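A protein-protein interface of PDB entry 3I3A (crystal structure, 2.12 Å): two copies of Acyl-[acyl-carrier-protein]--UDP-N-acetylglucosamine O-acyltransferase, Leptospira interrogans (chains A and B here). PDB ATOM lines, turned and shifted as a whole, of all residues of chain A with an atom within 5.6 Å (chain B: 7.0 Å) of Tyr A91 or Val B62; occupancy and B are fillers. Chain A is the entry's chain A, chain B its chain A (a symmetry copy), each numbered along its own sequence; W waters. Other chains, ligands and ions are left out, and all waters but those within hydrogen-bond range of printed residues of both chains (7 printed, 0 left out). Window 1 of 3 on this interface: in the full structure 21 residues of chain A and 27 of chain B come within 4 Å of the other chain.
The side-chain hydroxyl (OH) of Tyr A91 is in hydrogen-bond range of the backbone carbonyl oxygen (O) of Gly B60 (2.5 Å).
OE1 of Gln A59 is in hydrogen-bond range of OH of Tyr A91 (3.1 Å). The backbone carbonyl oxygen (O) of Glu B90 lies within hydrogen-bond range of the backbone NH (N) of Asn B115 (3.0 Å). The side-chain carboxylate of Glu A90 lies within salt-bridge range of the guanidinium group of Arg A89 (2.9 Å). The side-chain hydroxyl (OG) of Ser A92 lies within hydrogen-bond range of the backbone carbonyl oxygen (O) of Arg A89 (2.9 Å). The side-chain carboxylate (OE2) of Glu A90 is in hydrogen-bond range of a ring nitrogen (ND1) of His A58 (3.0 Å). The side-chain amide oxygen of Asn B93 sits close to a ring nitrogen (NE2) of His B95, at 2.9 Å.
Gln A59 touches Lys B44 (NE2 to CB, 3.4 Å). CG1 of Val B62 touches OE1 of Gln A59 (3.6 Å). Val B65 touches Arg A89 (CB to NH2, 3.8 Å). His B95 touches Arg A89. Val B65 touches Glu A90. Val B62 touches Tyr A91. CZ of Tyr A91 touches CD2 of Tyr B91 (3.5 Å). Asn A115 touches Asn B115 (ND2 to OD1, 3.5 Å).
His A58 touches none of the printed residues of chain B. Of the printed residues of chain B, Arg A89 touches Val B65 (3.8 Å) and His B95 (3.7 Å). Tyr A91 touches three residues of chain B. Printed residues of chain B within 4 Å of Asn A115: Asn B115 (3.5 Å). Of the printed residues of chain A, Lys B44 touches Gln A59 (3.4 Å). Ser B92 touches none of the printed residues of chain A.
Hydrophobic or aromatic side chains of chain B within 4 Å of the printed part of chain A: Val B62, Val B65, Tyr B91 and His B95. Of the 13 printed residues of chain A, 5 touch a printed residue of chain B. Printed residues of chain A that touch a printed residue of chain B: Gln A59, Arg A89, Glu A90, Tyr A91 and Asn A115. Hydrophobic or aromatic side chains of chain A within 4 Å of the printed part of chain B: Tyr A91. Along chain A the printed residues that touch a printed residue of chain B span positions 59 to 115. Among the printed residues, 9 pairs touch across the chains. Among the printed residues, no Asp or Glu carboxylate lies within 4 Å of a Lys or Arg side-chain nitrogen of the other chain.
Gln A59 touches Val B62, but with the chains exchanged Val A62 does not touch Gln B59 (11.7 Å). Tyr A91 touches Gly B60, but with the chains exchanged Gly A60 does not touch Tyr B91 (7.1 Å). Tyr B91 touches its own counterpart, Tyr A91. Asn A115 touches its own counterpart, Asn B115. Of the 9 pairs that touch across the chains among the printed residues, 2 have their exchanged pair printed and touching as well.
Water W2 bridges the side-chain carboxylate (OE2) of Glu A90 (2.6 Å) and the side-chain amino group (NZ) of Lys B44 (2.8 Å). Water W6 lies within hydrogen-bond range of ND2 of Asn A115 (2.6 Å) and O of Asn B115 (2.8 Å). Water W4 lies within hydrogen-bond range of OD1 of Asn A115 (2.7 Å) and OD1 of Asn B115 (2.7 Å). Water W1 bridges the side-chain amide oxygen of Asn A115 and the backbone carbonyl oxygen of Tyr B91. Water W7 lies within hydrogen-bond range of the backbone carbonyl oxygen of Glu A90 (2.7 Å), the side-chain amide nitrogen of Asn B93 (2.9 Å) and the backbone NH of Asn A115 (3.3 Å). Water W3 lies within hydrogen-bond range of OE1 of Glu A90 (2.7 Å), ND2 of Asn B93 (2.8 Å) and NE2 of His B95 (2.9 Å).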
ATOM      1  N   HIS A  58      14.698 -22.787 -33.495  1.00  0.00           N
ATOM      2  CA  HIS A  58      15.130 -23.216 -32.148  1.00  0.00           C
ATOM      3  C   HIS A  58      14.041 -24.020 -31.462  1.00  0.00           C
ATOM      4  O   HIS A  58      12.874 -23.948 -31.846  1.00  0.00           O
ATOM      5  CB  HIS A  58      15.496 -22.007 -31.272  1.00  0.00           C
ATOM      6  CG  HIS A  58      16.808 -21.370 -31.622  1.00  0.00           C
ATOM      7  ND1 HIS A  58      17.869 -21.322 -30.743  1.00  0.00           N
ATOM      8  CD2 HIS A  58      17.227 -20.750 -32.752  1.00  0.00           C
ATOM      9  CE1 HIS A  58      18.880 -20.687 -31.313  1.00  0.00           C
ATOM     10  NE2 HIS A  58      18.518 -20.331 -32.532  1.00  0.00           N
ATOM     11  N   GLN A  59      14.432 -24.764 -30.433  1.00  0.00           N
ATOM     12  CA  GLN A  59      13.537 -25.679 -29.727  1.00  0.00           C
ATOM     13  C   GLN A  59      12.134 -25.142 -29.444  1.00  0.00           C
ATOM     14  O   GLN A  59      11.968 -24.059 -28.877  1.00  0.00           O
ATOM     15  CB  GLN A  59      14.159 -26.161 -28.412  1.00  0.00           C
ATOM     16  CG  GLN A  59      13.762 -27.596 -28.129  1.00  0.00           C
ATOM     17  CD  GLN A  59      13.535 -27.903 -26.690  1.00  0.00           C
ATOM     18  OE1 GLN A  59      12.733 -27.255 -26.007  1.00  0.00           O
ATOM     19  NE2 GLN A  59      14.215 -28.925 -26.215  1.00  0.00           N
ATOM     20  N   GLY A  60      11.134 -25.926 -29.840  1.00  0.00           N
ATOM     21  CA  GLY A  60       9.752 -25.633 -29.505  1.00  0.00           C
ATOM     22  C   GLY A  60       9.071 -24.584 -30.369  1.00  0.00           C
ATOM     23  O   GLY A  60       7.893 -24.305 -30.172  1.00  0.00           O
ATOM     24  N   ALA A  61       9.798 -24.004 -31.321  1.00  0.00           N
ATOM     25  CA  ALA A  61       9.195 -23.060 -32.255  1.00  0.00           C
ATOM     26  C   ALA A  61       8.087 -23.763 -33.038  1.00  0.00           C
ATOM     27  O   ALA A  61       8.242 -24.919 -33.449  1.00  0.00           O
ATOM     28  CB  ALA A  61      10.242 -22.487 -33.200  1.00  0.00           C
ATOM     29  N   VAL A  62       6.958 -23.077 -33.206  1.00  0.00           N
ATOM     30  CA  VAL A  62       5.836 -23.626 -33.962  1.00  0.00           C
ATOM     31  C   VAL A  62       5.510 -22.755 -35.189  1.00  0.00           C
ATOM     32  O   VAL A  62       5.276 -21.550 -35.069  1.00  0.00           O
ATOM     33  CB  VAL A  62       4.600 -23.919 -33.065  1.00  0.00           C
ATOM     34  CG1 VAL A  62       4.902 -25.072 -32.099  1.00  0.00           C
ATOM     35  CG2 VAL A  62       4.136 -22.682 -32.303  1.00  0.00           C
ATOM     36  N   ARG A  89      13.432 -18.106 -32.537  1.00  0.00           N
ATOM     37  CA  ARG A  89      13.929 -18.542 -31.233  1.00  0.00           C
ATOM     38  C   ARG A  89      12.913 -19.432 -30.531  1.00  0.00           C
ATOM     39  O   ARG A  89      11.838 -19.715 -31.078  1.00  0.00           O
ATOM     40  CB  ARG A  89      14.321 -17.345 -30.360  1.00  0.00           C
ATOM     41  CG  ARG A  89      15.575 -16.584 -30.830  1.00  0.00           C
ATOM     42  CD  ARG A  89      16.761 -17.521 -31.044  1.00  0.00           C
ATOM     43  NE  ARG A  89      17.124 -18.264 -29.832  1.00  0.00           N
ATOM     44  CZ  ARG A  89      18.192 -18.011 -29.077  1.00  0.00           C
ATOM     45  NH1 ARG A  89      19.021 -17.031 -29.399  1.00  0.00           N
ATOM     46  NH2 ARG A  89      18.441 -18.749 -28.004  1.00  0.00           N
ATOM     47  N   GLU A  90      13.260 -19.858 -29.316  1.00  0.00           N
ATOM     48  CA  GLU A  90      12.536 -20.906 -28.621  1.00  0.00           C
ATOM     49  C   GLU A  90      11.084 -20.543 -28.333  1.00  0.00           C
ATOM     50  O   GLU A  90      10.808 -19.478 -27.794  1.00  0.00           O
ATOM     51  CB  GLU A  90      13.256 -21.264 -27.321  1.00  0.00           C
ATOM     52  CG  GLU A  90      14.561 -22.040 -27.519  1.00  0.00           C
ATOM     53  CD  GLU A  90      15.789 -21.170 -27.800  1.00  0.00           C
ATOM     54  OE1 GLU A  90      15.676 -19.921 -27.905  1.00  0.00           O
ATOM     55  OE2 GLU A  90      16.883 -21.762 -27.921  1.00  0.00           O
ATOM     56  N   TYR A  91      10.170 -21.441 -28.690  1.00  0.00           N
ATOM     57  CA  TYR A  91       8.723 -21.277 -28.440  1.00  0.00           C
ATOM     58  C   TYR A  91       8.104 -20.069 -29.158  1.00  0.00           C
ATOM     59  O   TYR A  91       6.977 -19.678 -28.850  1.00  0.00           O
ATOM     60  CB  TYR A  91       8.390 -21.275 -26.928  1.00  0.00           C
ATOM     61  CG  TYR A  91       8.966 -22.465 -26.212  1.00  0.00           C
ATOM     62  CD1 TYR A  91       9.944 -22.313 -25.230  1.00  0.00           C
ATOM     63  CD2 TYR A  91       8.566 -23.752 -26.545  1.00  0.00           C
ATOM     64  CE1 TYR A  91      10.500 -23.421 -24.596  1.00  0.00           C
ATOM     65  CE2 TYR A  91       9.116 -24.859 -25.917  1.00  0.00           C
ATOM     66  CZ  TYR A  91      10.085 -24.685 -24.952  1.00  0.00           C
ATOM     67  OH  TYR A  91      10.615 -25.792 -24.342  1.00  0.00           O
ATOM     68  N   SER A  92       8.841 -19.498 -30.117  1.00  0.00           N
ATOM     69  CA  SER A  92       8.274 -18.505 -31.040  1.00  0.00           C
ATOM     70  C   SER A  92       7.166 -19.205 -31.836  1.00  0.00           C
ATOM     71  O   SER A  92       7.214 -20.420 -32.062  1.00  0.00           O
ATOM     72  CB  SER A  92       9.334 -17.850 -31.943  1.00  0.00           C
ATOM     73  OG  SER A  92       9.847 -18.748 -32.917  1.00  0.00           O
ATOM     74  N   ASN A  93       6.184 -18.416 -32.264  1.00  0.00           N
ATOM     75  CA  ASN A  93       4.914 -18.937 -32.736  1.00  0.00           C
ATOM     76  C   ASN A  93       4.462 -18.164 -33.980  1.00  0.00           C
ATOM     77  O   ASN A  93       4.159 -16.972 -33.897  1.00  0.00           O
ATOM     78  CB  ASN A  93       3.898 -18.807 -31.586  1.00  0.00           C
ATOM     79  CG  ASN A  93       2.581 -19.499 -31.862  1.00  0.00           C
ATOM     80  OD1 ASN A  93       2.153 -19.629 -33.005  1.00  0.00           O
ATOM     81  ND2 ASN A  93       1.910 -19.928 -30.792  1.00  0.00           N
ATOM     82  N   GLY A 114      12.550 -15.458 -28.432  1.00  0.00           N
ATOM     83  CA  GLY A 114      11.782 -16.464 -27.705  1.00  0.00           C
ATOM     84  C   GLY A 114      10.388 -15.962 -27.364  1.00  0.00           C
ATOM     85  O   GLY A 114      10.205 -14.792 -27.017  1.00  0.00           O
ATOM     86  N   ASN A 115       9.403 -16.843 -27.486  1.00  0.00           N
ATOM     87  CA  ASN A 115       8.029 -16.523 -27.123  1.00  0.00           C
ATOM     88  C   ASN A 115       7.357 -15.445 -27.973  1.00  0.00           C
ATOM     89  O   ASN A 115       6.247 -15.044 -27.654  1.00  0.00           O
ATOM     90  CB  ASN A 115       7.926 -16.118 -25.635  1.00  0.00           C
ATOM     91  CG  ASN A 115       7.708 -17.292 -24.724  1.00  0.00           C
ATOM     92  OD1 ASN A 115       7.597 -18.428 -25.173  1.00  0.00           O
ATOM     93  ND2 ASN A 115       7.648 -17.028 -23.415  1.00  0.00           N
ATOM     94  N   SER A 116       8.021 -14.966 -29.021  1.00  0.00           N
ATOM     95  CA  SER A 116       7.412 -13.957 -29.897  1.00  0.00           C
ATOM     96  C   SER A 116       6.350 -14.599 -30.783  1.00  0.00           C
ATOM     97  O   SER A 116       6.401 -15.797 -31.055  1.00  0.00           O
ATOM     98  CB  SER A 116       8.454 -13.177 -30.710  1.00  0.00           C
ATOM     99  OG  SER A 116       9.138 -14.002 -31.647  1.00  0.00           O
ATOM    100  N   HIS B  42      10.559 -32.854 -21.678  1.00  0.00           N
ATOM    101  CA  HIS B  42      10.769 -31.815 -22.710  1.00  0.00           C
ATOM    102  C   HIS B  42      11.651 -30.648 -22.254  1.00  0.00           C
ATOM    103  O   HIS B  42      11.564 -29.541 -22.795  1.00  0.00           O
ATOM    104  CB  HIS B  42       9.433 -31.254 -23.231  1.00  0.00           C
ATOM    105  CG  HIS B  42       8.483 -32.302 -23.717  1.00  0.00           C
ATOM    106  ND1 HIS B  42       7.205 -32.430 -23.223  1.00  0.00           N
ATOM    107  CD2 HIS B  42       8.626 -33.276 -24.648  1.00  0.00           C
ATOM    108  CE1 HIS B  42       6.600 -33.438 -23.825  1.00  0.00           C
ATOM    109  NE2 HIS B  42       7.439 -33.967 -24.697  1.00  0.00           N
ATOM    110  N   VAL B  43      12.504 -30.901 -21.267  1.00  0.00           N
ATOM    111  CA  VAL B  43      13.427 -29.890 -20.748  1.00  0.00           C
ATOM    112  C   VAL B  43      14.716 -29.950 -21.563  1.00  0.00           C
ATOM    113  O   VAL B  43      15.149 -31.031 -21.957  1.00  0.00           O
ATOM    114  CB  VAL B  43      13.729 -30.098 -19.241  1.00  0.00           C
ATOM    115  CG1 VAL B  43      14.846 -29.167 -18.756  1.00  0.00           C
ATOM    116  CG2 VAL B  43      12.458 -29.911 -18.408  1.00  0.00           C
ATOM    117  N   LYS B  44      15.317 -28.788 -21.824  1.00  0.00           N
ATOM    118  CA  LYS B  44      16.608 -28.730 -22.504  1.00  0.00           C
ATOM    119  C   LYS B  44      17.690 -28.052 -21.663  1.00  0.00           C
ATOM    120  O   LYS B  44      17.538 -26.900 -21.240  1.00  0.00           O
ATOM    121  CB  LYS B  44      16.481 -28.048 -23.867  1.00  0.00           C
ATOM    122  CG  LYS B  44      17.685 -28.296 -24.794  1.00  0.00           C
ATOM    123  CD  LYS B  44      17.576 -27.454 -26.062  1.00  0.00           C
ATOM    124  CE  LYS B  44      18.805 -27.604 -26.947  1.00  0.00           C
ATOM    125  NZ  LYS B  44      18.600 -26.868 -28.237  1.00  0.00           N
ATOM    126  N   ILE B  45      18.770 -28.791 -21.417  1.00  0.00           N
ATOM    127  CA  ILE B  45      19.928 -28.280 -20.690  1.00  0.00           C
ATOM    128  C   ILE B  45      21.121 -28.212 -21.649  1.00  0.00           C
ATOM    129  O   ILE B  45      21.623 -29.242 -22.114  1.00  0.00           O
ATOM    130  CB  ILE B  45      20.287 -29.153 -19.448  1.00  0.00           C
ATOM    131  CG1 ILE B  45      19.052 -29.446 -18.566  1.00  0.00           C
ATOM    132  CG2 ILE B  45      21.433 -28.520 -18.660  1.00  0.00           C
ATOM    133  CD1 ILE B  45      18.485 -28.242 -17.772  1.00  0.00           C
ATOM    134  N   CYS B  46      21.567 -26.993 -21.941  1.00  0.00           N
ATOM    135  CA  CYS B  46      22.554 -26.771 -22.999  1.00  0.00           C
ATOM    136  C   CYS B  46      23.972 -26.830 -22.484  1.00  0.00           C
ATOM    137  O   CYS B  46      24.203 -26.692 -21.277  1.00  0.00           O
ATOM    138  CB  CYS B  46      22.321 -25.418 -23.667  1.00  0.00           C
ATOM    139  SG  CYS B  46      20.764 -25.311 -24.534  1.00  0.00           S
ATOM    140  N   PHE B  57      13.396 -28.449 -12.622  1.00  0.00           N
ATOM    141  CA  PHE B  57      13.152 -27.925 -13.954  1.00  0.00           C
ATOM    142  C   PHE B  57      11.849 -28.509 -14.469  1.00  0.00           C
ATOM    143  O   PHE B  57      11.775 -29.701 -14.762  1.00  0.00           O
ATOM    144  CB  PHE B  57      14.338 -28.238 -14.872  1.00  0.00           C
ATOM    145  CG  PHE B  57      15.629 -27.617 -14.405  1.00  0.00           C
ATOM    146  CD1 PHE B  57      16.430 -28.272 -13.470  1.00  0.00           C
ATOM    147  CD2 PHE B  57      16.030 -26.368 -14.876  1.00  0.00           C
ATOM    148  CE1 PHE B  57      17.613 -27.709 -13.020  1.00  0.00           C
ATOM    149  CE2 PHE B  57      17.223 -25.792 -14.423  1.00  0.00           C
ATOM    150  CZ  PHE B  57      18.016 -26.463 -13.500  1.00  0.00           C
ATOM    151  N   HIS B  58      10.823 -27.663 -14.552  1.00  0.00           N
ATOM    152  CA  HIS B  58       9.484 -28.086 -15.013  1.00  0.00           C
ATOM    153  C   HIS B  58       9.442 -28.196 -16.526  1.00  0.00           C
ATOM    154  O   HIS B  58      10.286 -27.627 -17.217  1.00  0.00           O
ATOM    155  CB  HIS B  58       8.399 -27.101 -14.546  1.00  0.00           C
ATOM    156  CG  HIS B  58       8.065 -27.204 -13.087  1.00  0.00           C
ATOM    157  ND1 HIS B  58       6.811 -27.561 -12.636  1.00  0.00           N
ATOM    158  CD2 HIS B  58       8.817 -26.990 -11.980  1.00  0.00           C
ATOM    159  CE1 HIS B  58       6.804 -27.549 -11.314  1.00  0.00           C
ATOM    160  NE2 HIS B  58       8.007 -27.207 -10.890  1.00  0.00           N
ATOM    161  N   GLN B  59       8.441 -28.912 -17.027  1.00  0.00           N
ATOM    162  CA  GLN B  59       8.310 -29.208 -18.453  1.00  0.00           C
ATOM    163  C   GLN B  59       8.608 -28.044 -19.398  1.00  0.00           C
ATOM    164  O   GLN B  59       8.047 -26.953 -19.262  1.00  0.00           O
ATOM    165  CB  GLN B  59       6.923 -29.771 -18.778  1.00  0.00           C
ATOM    166  CG  GLN B  59       7.013 -30.805 -19.882  1.00  0.00           C
ATOM    167  CD  GLN B  59       5.866 -30.800 -20.829  1.00  0.00           C
ATOM    168  OE1 GLN B  59       5.530 -29.776 -21.438  1.00  0.00           O
ATOM    169  NE2 GLN B  59       5.264 -31.959 -20.999  1.00  0.00           N
ATOM    170  N   GLY B  60       9.490 -28.303 -20.360  1.00  0.00           N
ATOM    171  CA  GLY B  60       9.761 -27.356 -21.427  1.00  0.00           C
ATOM    172  C   GLY B  60      10.705 -26.218 -21.077  1.00  0.00           C
ATOM    173  O   GLY B  60      11.011 -25.396 -21.933  1.00  0.00           O
ATOM    174  N   ALA B  61      11.168 -26.164 -19.830  1.00  0.00           N
ATOM    175  CA  ALA B  61      12.152 -25.162 -19.438  1.00  0.00           C
ATOM    176  C   ALA B  61      13.418 -25.344 -20.276  1.00  0.00           C
ATOM    177  O   ALA B  61      13.853 -26.476 -20.523  1.00  0.00           O
ATOM    178  CB  ALA B  61      12.471 -25.265 -17.953  1.00  0.00           C
ATOM    179  N   VAL B  62      13.981 -24.231 -20.743  1.00  0.00           N
ATOM    180  CA  VAL B  62      15.209 -24.270 -21.531  1.00  0.00           C
ATOM    181  C   VAL B  62      16.343 -23.496 -20.834  1.00  0.00           C
ATOM    182  O   VAL B  62      16.197 -22.318 -20.498  1.00  0.00           O
ATOM    183  CB  VAL B  62      14.984 -23.839 -23.008  1.00  0.00           C
ATOM    184  CG1 VAL B  62      14.126 -24.877 -23.742  1.00  0.00           C
ATOM    185  CG2 VAL B  62      14.361 -22.450 -23.114  1.00  0.00           C
ATOM    186  N   ILE B  63      17.465 -24.178 -20.613  1.00  0.00           N
ATOM    187  CA  ILE B  63      18.548 -23.656 -19.777  1.00  0.00           C
ATOM    188  C   ILE B  63      19.856 -23.543 -20.564  1.00  0.00           C
ATOM    189  O   ILE B  63      20.343 -24.530 -21.111  1.00  0.00           O
ATOM    190  CB  ILE B  63      18.790 -24.557 -18.522  1.00  0.00           C
ATOM    191  CG1 ILE B  63      17.510 -24.713 -17.680  1.00  0.00           C
ATOM    192  CG2 ILE B  63      19.965 -24.041 -17.681  1.00  0.00           C
ATOM    193  CD1 ILE B  63      16.904 -23.420 -17.131  1.00  0.00           C
ATOM    194  N   GLY B  64      20.413 -22.339 -20.614  1.00  0.00           N
ATOM    195  CA  GLY B  64      21.671 -22.103 -21.298  1.00  0.00           C
ATOM    196  C   GLY B  64      21.577 -21.995 -22.815  1.00  0.00           C
ATOM    197  O   GLY B  64      22.575 -22.206 -23.521  1.00  0.00           O
ATOM    198  N   VAL B  65      20.399 -21.650 -23.322  1.00  0.00           N
ATOM    199  CA  VAL B  65      20.218 -21.453 -24.765  1.00  0.00           C
ATOM    200  C   VAL B  65      21.084 -20.277 -25.276  1.00  0.00           C
ATOM    201  O   VAL B  65      21.510 -19.440 -24.488  1.00  0.00           O
ATOM    202  CB  VAL B  65      18.724 -21.284 -25.134  1.00  0.00           C
ATOM    203  CG1 VAL B  65      17.963 -22.585 -24.878  1.00  0.00           C
ATOM    204  CG2 VAL B  65      18.090 -20.160 -24.337  1.00  0.00           C
ATOM    205  N   PHE B  88      12.511 -23.643 -11.735  1.00  0.00           N
ATOM    206  CA  PHE B  88      12.276 -23.103 -13.059  1.00  0.00           C
ATOM    207  C   PHE B  88      10.984 -23.711 -13.570  1.00  0.00           C
ATOM    208  O   PHE B  88      10.907 -24.927 -13.795  1.00  0.00           O
ATOM    209  CB  PHE B  88      13.440 -23.450 -13.995  1.00  0.00           C
ATOM    210  CG  PHE B  88      14.759 -22.923 -13.530  1.00  0.00           C
ATOM    211  CD1 PHE B  88      15.483 -23.587 -12.532  1.00  0.00           C
ATOM    212  CD2 PHE B  88      15.284 -21.765 -14.074  1.00  0.00           C
ATOM    213  CE1 PHE B  88      16.701 -23.098 -12.096  1.00  0.00           C
ATOM    214  CE2 PHE B  88      16.501 -21.269 -13.640  1.00  0.00           C
ATOM    215  CZ  PHE B  88      17.209 -21.937 -12.646  1.00  0.00           C
ATOM    216  N   ARG B  89       9.970 -22.864 -13.735  1.00  0.00           N
ATOM    217  CA  ARG B  89       8.642 -23.328 -14.130  1.00  0.00           C
ATOM    218  C   ARG B  89       8.564 -23.546 -15.635  1.00  0.00           C
ATOM    219  O   ARG B  89       9.555 -23.350 -16.352  1.00  0.00           O
ATOM    220  CB  ARG B  89       7.551 -22.367 -13.647  1.00  0.00           C
ATOM    221  CG  ARG B  89       7.332 -22.347 -12.123  1.00  0.00           C
ATOM    222  CD  ARG B  89       7.116 -23.751 -11.562  1.00  0.00           C
ATOM    223  NE  ARG B  89       5.963 -24.431 -12.165  1.00  0.00           N
ATOM    224  CZ  ARG B  89       4.794 -24.627 -11.558  1.00  0.00           C
ATOM    225  NH1 ARG B  89       4.604 -24.199 -10.320  1.00  0.00           N
ATOM    226  NH2 ARG B  89       3.816 -25.265 -12.184  1.00  0.00           N
ATOM    227  N   GLU B  90       7.380 -23.941 -16.101  1.00  0.00           N
ATOM    228  CA  GLU B  90       7.198 -24.436 -17.454  1.00  0.00           C
ATOM    229  C   GLU B  90       7.533 -23.400 -18.520  1.00  0.00           C
ATOM    230  O   GLU B  90       7.048 -22.277 -18.465  1.00  0.00           O
ATOM    231  CB  GLU B  90       5.768 -24.938 -17.639  1.00  0.00           C
ATOM    232  CG  GLU B  90       5.465 -26.255 -16.919  1.00  0.00           C
ATOM    233  CD  GLU B  90       5.077 -26.107 -15.445  1.00  0.00           C
ATOM    234  OE1 GLU B  90       5.073 -24.974 -14.897  1.00  0.00           O
ATOM    235  OE2 GLU B  90       4.777 -27.155 -14.833  1.00  0.00           O
ATOM    236  N   TYR B  91       8.357 -23.795 -19.486  1.00  0.00           N
ATOM    237  CA  TYR B  91       8.747 -22.940 -20.628  1.00  0.00           C
ATOM    238  C   TYR B  91       9.515 -21.675 -20.219  1.00  0.00           C
ATOM    239  O   TYR B  91       9.687 -20.766 -21.032  1.00  0.00           O
ATOM    240  CB  TYR B  91       7.543 -22.607 -21.543  1.00  0.00           C
ATOM    241  CG  TYR B  91       6.794 -23.836 -21.976  1.00  0.00           C
ATOM    242  CD1 TYR B  91       5.472 -24.051 -21.585  1.00  0.00           C
ATOM    243  CD2 TYR B  91       7.416 -24.810 -22.743  1.00  0.00           C
ATOM    244  CE1 TYR B  91       4.795 -25.208 -21.959  1.00  0.00           C
ATOM    245  CE2 TYR B  91       6.747 -25.964 -23.119  1.00  0.00           C
ATOM    246  CZ  TYR B  91       5.443 -26.159 -22.717  1.00  0.00           C
ATOM    247  OH  TYR B  91       4.797 -27.305 -23.100  1.00  0.00           O
ATOM    248  N   SER B  92       9.981 -21.634 -18.966  1.00  0.00           N
ATOM    249  CA  SER B  92      10.935 -20.606 -18.528  1.00  0.00           C
ATOM    250  C   SER B  92      12.211 -20.787 -19.358  1.00  0.00           C
ATOM    251  O   SER B  92      12.534 -21.898 -19.796  1.00  0.00           O
ATOM    252  CB  SER B  92      11.201 -20.637 -17.013  1.00  0.00           C
ATOM    253  OG  SER B  92      11.950 -21.777 -16.617  1.00  0.00           O
ATOM    254  N   ASN B  93      12.929 -19.684 -19.552  1.00  0.00           N
ATOM    255  CA  ASN B  93      13.966 -19.594 -20.564  1.00  0.00           C
ATOM    256  C   ASN B  93      15.182 -18.849 -20.001  1.00  0.00           C
ATOM    257  O   ASN B  93      15.100 -17.655 -19.709  1.00  0.00           O
ATOM    258  CB  ASN B  93      13.369 -18.868 -21.783  1.00  0.00           C
ATOM    259  CG  ASN B  93      14.270 -18.884 -22.997  1.00  0.00           C
ATOM    260  OD1 ASN B  93      15.492 -18.927 -22.887  1.00  0.00           O
ATOM    261  ND2 ASN B  93      13.661 -18.818 -24.181  1.00  0.00           N
ATOM    262  N   ILE B  94      16.300 -19.557 -19.840  1.00  0.00           N
ATOM    263  CA  ILE B  94      17.513 -18.952 -19.290  1.00  0.00           C
ATOM    264  C   ILE B  94      18.638 -18.996 -20.319  1.00  0.00           C
ATOM    265  O   ILE B  94      19.004 -20.066 -20.815  1.00  0.00           O
ATOM    266  CB  ILE B  94      17.994 -19.669 -17.983  1.00  0.00           C
ATOM    267  CG1 ILE B  94      16.832 -19.984 -17.018  1.00  0.00           C
ATOM    268  CG2 ILE B  94      19.124 -18.884 -17.312  1.00  0.00           C
ATOM    269  CD1 ILE B  94      16.124 -18.770 -16.373  1.00  0.00           C
ATOM    270  N   HIS B  95      19.182 -17.822 -20.638  1.00  0.00           N
ATOM    271  CA  HIS B  95      20.242 -17.705 -21.635  1.00  0.00           C
ATOM    272  C   HIS B  95      21.619 -17.699 -20.986  1.00  0.00           C
ATOM    273  O   HIS B  95      21.792 -17.134 -19.906  1.00  0.00           O
ATOM    274  CB  HIS B  95      20.031 -16.450 -22.482  1.00  0.00           C
ATOM    275  CG  HIS B  95      18.868 -16.553 -23.418  1.00  0.00           C
ATOM    276  ND1 HIS B  95      18.895 -16.054 -24.699  1.00  0.00           N
ATOM    277  CD2 HIS B  95      17.654 -17.134 -23.269  1.00  0.00           C
ATOM    278  CE1 HIS B  95      17.741 -16.307 -25.294  1.00  0.00           C
ATOM    279  NE2 HIS B  95      16.973 -16.968 -24.451  1.00  0.00           N
ATOM    280  N   ASN B 115       7.077 -19.275 -18.435  1.00  0.00           N
ATOM    281  CA  ASN B 115       7.315 -18.305 -19.496  1.00  0.00           C
ATOM    282  C   ASN B 115       8.239 -17.144 -19.130  1.00  0.00           C
ATOM    283  O   ASN B 115       8.393 -16.233 -19.930  1.00  0.00           O
ATOM    284  CB  ASN B 115       5.985 -17.730 -20.033  1.00  0.00           C
ATOM    285  CG  ASN B 115       5.406 -18.549 -21.152  1.00  0.00           C
ATOM    286  OD1 ASN B 115       5.989 -19.541 -21.577  1.00  0.00           O
ATOM    287  ND2 ASN B 115       4.234 -18.138 -21.647  1.00  0.00           N
HETATM  288  O   HOH W   1       9.484 -19.164 -23.343  1.00  0.00           O
HETATM  289  O   HOH W   2      17.832 -24.174 -28.182  1.00  0.00           O
HETATM  290  O   HOH W   3      14.926 -17.752 -26.396  1.00  0.00           O
HETATM  291  O   HOH W   4       5.983 -20.263 -24.134  1.00  0.00           O
HETATM  292  O   HOH W   5       7.678 -13.824 -22.115  1.00  0.00           O
HETATM  293  O   HOH W   6       9.961 -16.732 -22.227  1.00  0.00           O
HETATM  294  O   HOH W   7      11.026 -18.534 -25.233  1.00  0.00           O
